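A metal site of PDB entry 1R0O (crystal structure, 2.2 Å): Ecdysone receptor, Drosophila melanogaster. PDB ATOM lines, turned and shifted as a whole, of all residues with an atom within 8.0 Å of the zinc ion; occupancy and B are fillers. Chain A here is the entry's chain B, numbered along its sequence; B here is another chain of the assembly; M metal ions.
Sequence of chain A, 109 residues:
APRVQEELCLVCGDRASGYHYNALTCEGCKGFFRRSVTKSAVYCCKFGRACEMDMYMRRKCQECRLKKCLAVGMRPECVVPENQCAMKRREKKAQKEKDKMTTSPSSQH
The side-chain sulfur (SG) of Cys 12 of chain A lies close to the backbone NH (N) of Asp 14, 3.3 Å away. NH1 of Arg 58 sits close to SG of Cys 26. The guanidinium group of Arg 65 sits close to the side-chain sulfur of Cys 29 (3.5 Å). The side-chain sulfur of Cys 26 sits close to the backbone NH of Gly 28 (3.5 Å). The side-chain sulfur (SG) of Cys 9 sits close to the backbone NH (N) of Val 11 (3.2 Å). SG of Cys 12 of chain A lies close to NH1 of Arg 58 (3.1 Å). The backbone NH (N) of Cys 9 sits at hydrogen-bond distance from the backbone carbonyl oxygen (O) of Asp 14.
Within 4 Å of the zinc ion: Cys 9, Cys 12 of chain A, Cys 26 and Cys 29. Along chain A the residues within 4 Å of the zinc ion span positions 9 to 29.
The zinc ion is bound by SG of Cys 29 (2.3 Å), SG of Cys 12 of chain A (2.3 Å), SG of Cys 26 (2.4 Å) and SG of Cys 9 (2.6 Å). The zinc ion has four donor atoms within binding distance.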
ATOM      1  N   LEU A   8     -33.854 -16.154  14.975  1.00  0.00           N
ATOM      2  CA  LEU A   8     -34.293 -16.645  13.669  1.00  0.00           C
ATOM      3  C   LEU A   8     -34.048 -15.843  12.407  1.00  0.00           C
ATOM      4  O   LEU A   8     -34.508 -14.706  12.244  1.00  0.00           O
ATOM      5  CB  LEU A   8     -35.771 -17.001  13.738  1.00  0.00           C
ATOM      6  CG  LEU A   8     -36.124 -18.362  14.354  1.00  0.00           C
ATOM      7  CD1 LEU A   8     -35.207 -18.702  15.533  1.00  0.00           C
ATOM      8  CD2 LEU A   8     -37.599 -18.373  14.762  1.00  0.00           C
ATOM      9  N   CYS A   9     -33.330 -16.471  11.494  1.00  0.00           N
ATOM     10  CA  CYS A   9     -33.046 -15.900  10.199  1.00  0.00           C
ATOM     11  C   CYS A   9     -34.385 -16.017   9.458  1.00  0.00           C
ATOM     12  O   CYS A   9     -34.995 -17.078   9.447  1.00  0.00           O
ATOM     13  CB  CYS A   9     -31.960 -16.719   9.511  1.00  0.00           C
ATOM     14  SG  CYS A   9     -31.941 -16.561   7.718  1.00  0.00           S
ATOM     15  N   LEU A  10     -34.841 -14.927   8.836  1.00  0.00           N
ATOM     16  CA  LEU A  10     -36.106 -14.951   8.125  1.00  0.00           C
ATOM     17  C   LEU A  10     -36.089 -15.866   6.911  1.00  0.00           C
ATOM     18  O   LEU A  10     -37.129 -16.250   6.392  1.00  0.00           O
ATOM     19  CB  LEU A  10     -36.514 -13.548   7.695  1.00  0.00           C
ATOM     20  CG  LEU A  10     -36.843 -12.654   8.888  1.00  0.00           C
ATOM     21  CD1 LEU A  10     -36.938 -11.189   8.451  1.00  0.00           C
ATOM     22  CD2 LEU A  10     -38.155 -13.138   9.528  1.00  0.00           C
ATOM     23  N   VAL A  11     -34.881 -16.213   6.471  1.00  0.00           N
ATOM     24  CA  VAL A  11     -34.751 -17.082   5.321  1.00  0.00           C
ATOM     25  C   VAL A  11     -34.766 -18.581   5.639  1.00  0.00           C
ATOM     26  O   VAL A  11     -35.639 -19.309   5.158  1.00  0.00           O
ATOM     27  CB  VAL A  11     -33.443 -16.788   4.533  1.00  0.00           C
ATOM     28  CG1 VAL A  11     -33.310 -17.749   3.359  1.00  0.00           C
ATOM     29  CG2 VAL A  11     -33.421 -15.355   4.054  1.00  0.00           C
ATOM     30  N   CYS A  12     -33.818 -19.027   6.468  1.00  0.00           N
ATOM     31  CA  CYS A  12     -33.686 -20.451   6.757  1.00  0.00           C
ATOM     32  C   CYS A  12     -34.017 -20.975   8.154  1.00  0.00           C
ATOM     33  O   CYS A  12     -33.998 -22.177   8.366  1.00  0.00           O
ATOM     34  CB  CYS A  12     -32.268 -20.890   6.420  1.00  0.00           C
ATOM     35  SG  CYS A  12     -31.068 -20.362   7.662  1.00  0.00           S
ATOM     36  N   GLY A  13     -34.298 -20.087   9.102  1.00  0.00           N
ATOM     37  CA  GLY A  13     -34.598 -20.523  10.465  1.00  0.00           C
ATOM     38  C   GLY A  13     -33.389 -20.830  11.340  1.00  0.00           C
ATOM     39  O   GLY A  13     -33.557 -21.234  12.500  1.00  0.00           O
ATOM     40  N   ASP A  14     -32.184 -20.669  10.802  1.00  0.00           N
ATOM     41  CA  ASP A  14     -30.960 -20.879  11.574  1.00  0.00           C
ATOM     42  C   ASP A  14     -30.968 -19.691  12.551  1.00  0.00           C
ATOM     43  O   ASP A  14     -31.870 -18.859  12.505  1.00  0.00           O
ATOM     44  CB  ASP A  14     -29.737 -20.803  10.653  1.00  0.00           C
ATOM     45  CG  ASP A  14     -28.431 -21.236  11.319  1.00  0.00           C
ATOM     46  OD1 ASP A  14     -27.408 -21.295  10.606  1.00  0.00           O
ATOM     47  OD2 ASP A  14     -28.420 -21.520  12.546  1.00  0.00           O
ATOM     48  N   ARG A  15     -29.974 -19.590  13.423  1.00  0.00           N
ATOM     49  CA  ARG A  15     -29.947 -18.464  14.345  1.00  0.00           C
ATOM     50  C   ARG A  15     -29.451 -17.195  13.629  1.00  0.00           C
ATOM     51  O   ARG A  15     -28.399 -17.202  13.000  1.00  0.00           O
ATOM     52  CB  ARG A  15     -29.060 -18.786  15.556  1.00  0.00           C
ATOM     53  CG  ARG A  15     -27.603 -19.092  15.227  1.00  0.00           C
ATOM     54  CD  ARG A  15     -27.158 -20.502  15.700  1.00  0.00           C
ATOM     55  NE  ARG A  15     -27.005 -20.595  17.153  1.00  0.00           N
ATOM     56  CZ  ARG A  15     -26.606 -21.687  17.806  1.00  0.00           C
ATOM     57  NH1 ARG A  15     -26.293 -22.800  17.144  1.00  0.00           N
ATOM     58  NH2 ARG A  15     -26.516 -21.673  19.131  1.00  0.00           N
ATOM     59  N   ALA A  16     -30.227 -16.112  13.694  1.00  0.00           N
ATOM     60  CA  ALA A  16     -29.801 -14.871  13.051  1.00  0.00           C
ATOM     61  C   ALA A  16     -28.663 -14.222  13.853  1.00  0.00           C
ATOM     62  O   ALA A  16     -28.624 -14.325  15.070  1.00  0.00           O
ATOM     63  CB  ALA A  16     -30.981 -13.896  12.943  1.00  0.00           C
ATOM     64  N   LEU A  24     -33.268  -9.575   9.123  1.00  0.00           N
ATOM     65  CA  LEU A  24     -32.748 -10.423  10.187  1.00  0.00           C
ATOM     66  C   LEU A  24     -32.407 -11.779   9.570  1.00  0.00           C
ATOM     67  O   LEU A  24     -33.303 -12.542   9.210  1.00  0.00           O
ATOM     68  CB  LEU A  24     -33.824 -10.561  11.283  1.00  0.00           C
ATOM     69  CG  LEU A  24     -33.385 -11.152  12.627  1.00  0.00           C
ATOM     70  CD1 LEU A  24     -32.203 -10.383  13.151  1.00  0.00           C
ATOM     71  CD2 LEU A  24     -34.541 -11.130  13.629  1.00  0.00           C
ATOM     72  N   THR A  25     -31.119 -12.075   9.459  1.00  0.00           N
ATOM     73  CA  THR A  25     -30.654 -13.312   8.825  1.00  0.00           C
ATOM     74  C   THR A  25     -29.408 -13.922   9.498  1.00  0.00           C
ATOM     75  O   THR A  25     -28.775 -13.276  10.335  1.00  0.00           O
ATOM     76  CB  THR A  25     -30.340 -13.015   7.341  1.00  0.00           C
ATOM     77  OG1 THR A  25     -29.405 -11.923   7.257  1.00  0.00           O
ATOM     78  CG2 THR A  25     -31.602 -12.616   6.591  1.00  0.00           C
ATOM     79  N   CYS A  26     -29.053 -15.145   9.105  1.00  0.00           N
ATOM     80  CA  CYS A  26     -27.886 -15.826   9.694  1.00  0.00           C
ATOM     81  C   CYS A  26     -26.623 -15.535   8.878  1.00  0.00           C
ATOM     82  O   CYS A  26     -26.695 -14.924   7.816  1.00  0.00           O
ATOM     83  CB  CYS A  26     -28.132 -17.339   9.758  1.00  0.00           C
ATOM     84  SG  CYS A  26     -28.103 -18.208   8.142  1.00  0.00           S
ATOM     85  N   GLU A  27     -25.470 -15.990   9.369  1.00  0.00           N
ATOM     86  CA  GLU A  27     -24.230 -15.753   8.626  1.00  0.00           C
ATOM     87  C   GLU A  27     -24.269 -16.429   7.260  1.00  0.00           C
ATOM     88  O   GLU A  27     -23.829 -15.860   6.256  1.00  0.00           O
ATOM     89  CB  GLU A  27     -23.011 -16.235   9.420  1.00  0.00           C
ATOM     90  CG  GLU A  27     -22.564 -15.263  10.516  1.00  0.00           C
ATOM     91  CD  GLU A  27     -22.282 -13.871   9.994  1.00  0.00           C
ATOM     92  OE1 GLU A  27     -21.468 -13.717   9.040  1.00  0.00           O
ATOM     93  OE2 GLU A  27     -22.873 -12.914  10.525  1.00  0.00           O
ATOM     94  N   GLY A  28     -24.809 -17.634   7.207  1.00  0.00           N
ATOM     95  CA  GLY A  28     -24.907 -18.335   5.948  1.00  0.00           C
ATOM     96  C   GLY A  28     -25.649 -17.536   4.898  1.00  0.00           C
ATOM     97  O   GLY A  28     -25.134 -17.323   3.811  1.00  0.00           O
ATOM     98  N   CYS A  29     -26.846 -17.056   5.216  1.00  0.00           N
ATOM     99  CA  CYS A  29     -27.631 -16.292   4.249  1.00  0.00           C
ATOM    100  C   CYS A  29     -27.022 -14.925   3.934  1.00  0.00           C
ATOM    101  O   CYS A  29     -27.124 -14.415   2.810  1.00  0.00           O
ATOM    102  CB  CYS A  29     -29.069 -16.184   4.745  1.00  0.00           C
ATOM    103  SG  CYS A  29     -29.875 -17.808   4.778  1.00  0.00           S
ATOM    104  N   LYS A  30     -26.372 -14.326   4.920  1.00  0.00           N
ATOM    105  CA  LYS A  30     -25.714 -13.047   4.723  1.00  0.00           C
ATOM    106  C   LYS A  30     -24.688 -13.225   3.611  1.00  0.00           C
ATOM    107  O   LYS A  30     -24.682 -12.499   2.619  1.00  0.00           O
ATOM    108  CB  LYS A  30     -25.020 -12.642   6.020  1.00  0.00           C
ATOM    109  CG  LYS A  30     -24.018 -11.522   5.901  1.00  0.00           C
ATOM    110  CD  LYS A  30     -23.267 -11.397   7.225  1.00  0.00           C
ATOM    111  CE  LYS A  30     -21.965 -10.621   7.090  1.00  0.00           C
ATOM    112  NZ  LYS A  30     -20.989 -11.053   8.122  1.00  0.00           N
ATOM    113  N   PHE A  32     -24.390 -15.825   1.522  1.00  0.00           N
ATOM    114  CA  PHE A  32     -24.952 -16.319   0.274  1.00  0.00           C
ATOM    115  C   PHE A  32     -25.504 -15.152  -0.499  1.00  0.00           C
ATOM    116  O   PHE A  32     -25.360 -15.066  -1.713  1.00  0.00           O
ATOM    117  CB  PHE A  32     -26.069 -17.339   0.514  1.00  0.00           C
ATOM    118  CG  PHE A  32     -26.851 -17.676  -0.730  1.00  0.00           C
ATOM    119  CD1 PHE A  32     -26.345 -18.568  -1.682  1.00  0.00           C
ATOM    120  CD2 PHE A  32     -28.089 -17.092  -0.978  1.00  0.00           C
ATOM    121  CE1 PHE A  32     -27.057 -18.839  -2.850  1.00  0.00           C
ATOM    122  CE2 PHE A  32     -28.805 -17.359  -2.133  1.00  0.00           C
ATOM    123  CZ  PHE A  32     -28.289 -18.237  -3.071  1.00  0.00           C
ATOM    124  N   MET A  53     -37.351 -23.286   2.516  1.00  0.00           N
ATOM    125  CA  MET A  53     -36.041 -23.189   3.140  1.00  0.00           C
ATOM    126  C   MET A  53     -35.902 -23.629   4.605  1.00  0.00           C
ATOM    127  O   MET A  53     -36.795 -23.406   5.434  1.00  0.00           O
ATOM    128  CB  MET A  53     -35.518 -21.748   3.023  1.00  0.00           C
ATOM    129  CG  MET A  53     -35.236 -21.284   1.615  1.00  0.00           C
ATOM    130  SD  MET A  53     -34.052 -22.317   0.784  1.00  0.00           S
ATOM    131  CE  MET A  53     -32.655 -21.596   1.376  1.00  0.00           C
ATOM    132  N   ASP A  54     -34.777 -24.267   4.900  1.00  0.00           N
ATOM    133  CA  ASP A  54     -34.393 -24.721   6.239  1.00  0.00           C
ATOM    134  C   ASP A  54     -32.883 -24.925   6.178  1.00  0.00           C
ATOM    135  O   ASP A  54     -32.301 -24.689   5.141  1.00  0.00           O
ATOM    136  CB  ASP A  54     -35.113 -26.012   6.676  1.00  0.00           C
ATOM    137  CG  ASP A  54     -34.855 -27.175   5.738  1.00  0.00           C
ATOM    138  OD1 ASP A  54     -33.707 -27.357   5.268  1.00  0.00           O
ATOM    139  OD2 ASP A  54     -35.822 -27.919   5.490  1.00  0.00           O
ATOM    140  N   MET A  55     -32.243 -25.328   7.267  1.00  0.00           N
ATOM    141  CA  MET A  55     -30.777 -25.451   7.213  1.00  0.00           C
ATOM    142  C   MET A  55     -30.231 -26.487   6.240  1.00  0.00           C
ATOM    143  O   MET A  55     -29.053 -26.464   5.891  1.00  0.00           O
ATOM    144  CB  MET A  55     -30.244 -25.682   8.610  1.00  0.00           C
ATOM    145  CG  MET A  55     -30.362 -24.438   9.454  1.00  0.00           C
ATOM    146  SD  MET A  55     -29.962 -24.705  11.139  1.00  0.00           S
ATOM    147  CE  MET A  55     -28.136 -25.134  10.999  1.00  0.00           C
ATOM    148  N   ARG A  58     -31.317 -24.931   2.242  1.00  0.00           N
ATOM    149  CA  ARG A  58     -30.613 -23.719   1.840  1.00  0.00           C
ATOM    150  C   ARG A  58     -29.378 -24.004   1.028  1.00  0.00           C
ATOM    151  O   ARG A  58     -29.021 -23.203   0.173  1.00  0.00           O
ATOM    152  CB  ARG A  58     -30.233 -22.851   3.058  1.00  0.00           C
ATOM    153  CG  ARG A  58     -29.009 -23.300   3.835  1.00  0.00           C
ATOM    154  CD  ARG A  58     -28.932 -22.554   5.159  1.00  0.00           C
ATOM    155  NE  ARG A  58     -27.703 -22.865   5.864  1.00  0.00           N
ATOM    156  CZ  ARG A  58     -27.402 -22.463   7.105  1.00  0.00           C
ATOM    157  NH1 ARG A  58     -28.263 -21.741   7.826  1.00  0.00           N
ATOM    158  NH2 ARG A  58     -26.219 -22.794   7.620  1.00  0.00           N
ATOM    159  N   ARG A  65     -33.302 -20.199  -2.557  1.00  0.00           N
ATOM    160  CA  ARG A  65     -32.729 -19.517  -1.388  1.00  0.00           C
ATOM    161  C   ARG A  65     -32.584 -18.021  -1.698  1.00  0.00           C
ATOM    162  O   ARG A  65     -32.908 -17.183  -0.854  1.00  0.00           O
ATOM    163  CB  ARG A  65     -31.355 -20.080  -1.039  1.00  0.00           C
ATOM    164  CG  ARG A  65     -30.737 -19.464   0.194  1.00  0.00           C
ATOM    165  CD  ARG A  65     -29.351 -20.045   0.438  1.00  0.00           C
ATOM    166  NE  ARG A  65     -28.834 -19.703   1.766  1.00  0.00           N
ATOM    167  CZ  ARG A  65     -27.684 -20.134   2.256  1.00  0.00           C
ATOM    168  NH1 ARG A  65     -26.899 -20.920   1.534  1.00  0.00           N
ATOM    169  NH2 ARG A  65     -27.329 -19.796   3.479  1.00  0.00           N
ATOM    170  N   CYS A  69     -34.401 -14.915   0.172  1.00  0.00           N
ATOM    171  CA  CYS A  69     -33.604 -13.797   0.678  1.00  0.00           C
ATOM    172  C   CYS A  69     -34.256 -12.465   0.301  1.00  0.00           C
ATOM    173  O   CYS A  69     -34.389 -11.565   1.133  1.00  0.00           O
ATOM    174  CB  CYS A  69     -32.201 -13.809   0.089  1.00  0.00           C
ATOM    175  SG  CYS A  69     -31.067 -15.015   0.770  1.00  0.00           S
ATOM    176  N   MET A  74     -33.971  -8.594   2.005  1.00  0.00           N
ATOM    177  CA  MET A  74     -32.545  -8.309   1.867  1.00  0.00           C
ATOM    178  C   MET A  74     -32.477  -7.451   0.614  1.00  0.00           C
ATOM    179  O   MET A  74     -33.087  -7.787  -0.405  1.00  0.00           O
ATOM    180  CB  MET A  74     -31.740  -9.605   1.724  1.00  0.00           C
ATOM    181  CG  MET A  74     -31.817 -10.518   2.953  1.00  0.00           C
ATOM    182  SD  MET A  74     -30.696 -11.942   2.901  1.00  0.00           S
ATOM    183  CE  MET A  74     -29.176 -11.216   3.526  1.00  0.00           C
ATOM    184  P    DG B  12     -24.245 -22.342   4.224  1.00  0.00           P
ATOM    185  OP1  DG B  12     -25.167 -23.389   4.750  1.00  0.00           O
ATOM    186  OP2  DG B  12     -24.818 -21.145   3.558  1.00  0.00           O
ATOM    187  O5'  DG B  12     -23.326 -21.836   5.423  1.00  0.00           O
ATOM    188  C5'  DG B  12     -22.618 -22.785   6.203  1.00  0.00           C
ATOM    189  C4'  DG B  12     -21.596 -22.099   7.076  1.00  0.00           C
ATOM    190  O4'  DG B  12     -20.561 -21.538   6.235  1.00  0.00           O
ATOM    191  C3'  DG B  12     -22.103 -20.939   7.936  1.00  0.00           C
ATOM    192  O3'  DG B  12     -21.350 -20.916   9.140  1.00  0.00           O
ATOM    193  C2'  DG B  12     -21.708 -19.711   7.128  1.00  0.00           C
ATOM    194  C1'  DG B  12     -20.378 -20.189   6.579  1.00  0.00           C
ATOM    195  N9   DG B  12     -19.831 -19.509   5.417  1.00  0.00           N
ATOM    196  C8   DG B  12     -20.486 -18.862   4.393  1.00  0.00           C
ATOM    197  N7   DG B  12     -19.662 -18.342   3.513  1.00  0.00           N
ATOM    198  C5   DG B  12     -18.394 -18.659   3.993  1.00  0.00           C
ATOM    199  C6   DG B  12     -17.114 -18.368   3.482  1.00  0.00           C
ATOM    200  O6   DG B  12     -16.814 -17.732   2.463  1.00  0.00           O
ATOM    201  N1   DG B  12     -16.103 -18.889   4.291  1.00  0.00           N
ATOM    202  C2   DG B  12     -16.311 -19.603   5.444  1.00  0.00           C
ATOM    203  N2   DG B  12     -15.220 -20.015   6.104  1.00  0.00           N
ATOM    204  N3   DG B  12     -17.498 -19.883   5.925  1.00  0.00           N
ATOM    205  C4   DG B  12     -18.486 -19.387   5.153  1.00  0.00           C
HETATM  206 ZN    ZN M   1     -30.204 -18.291   6.968  1.00  0.00          ZN
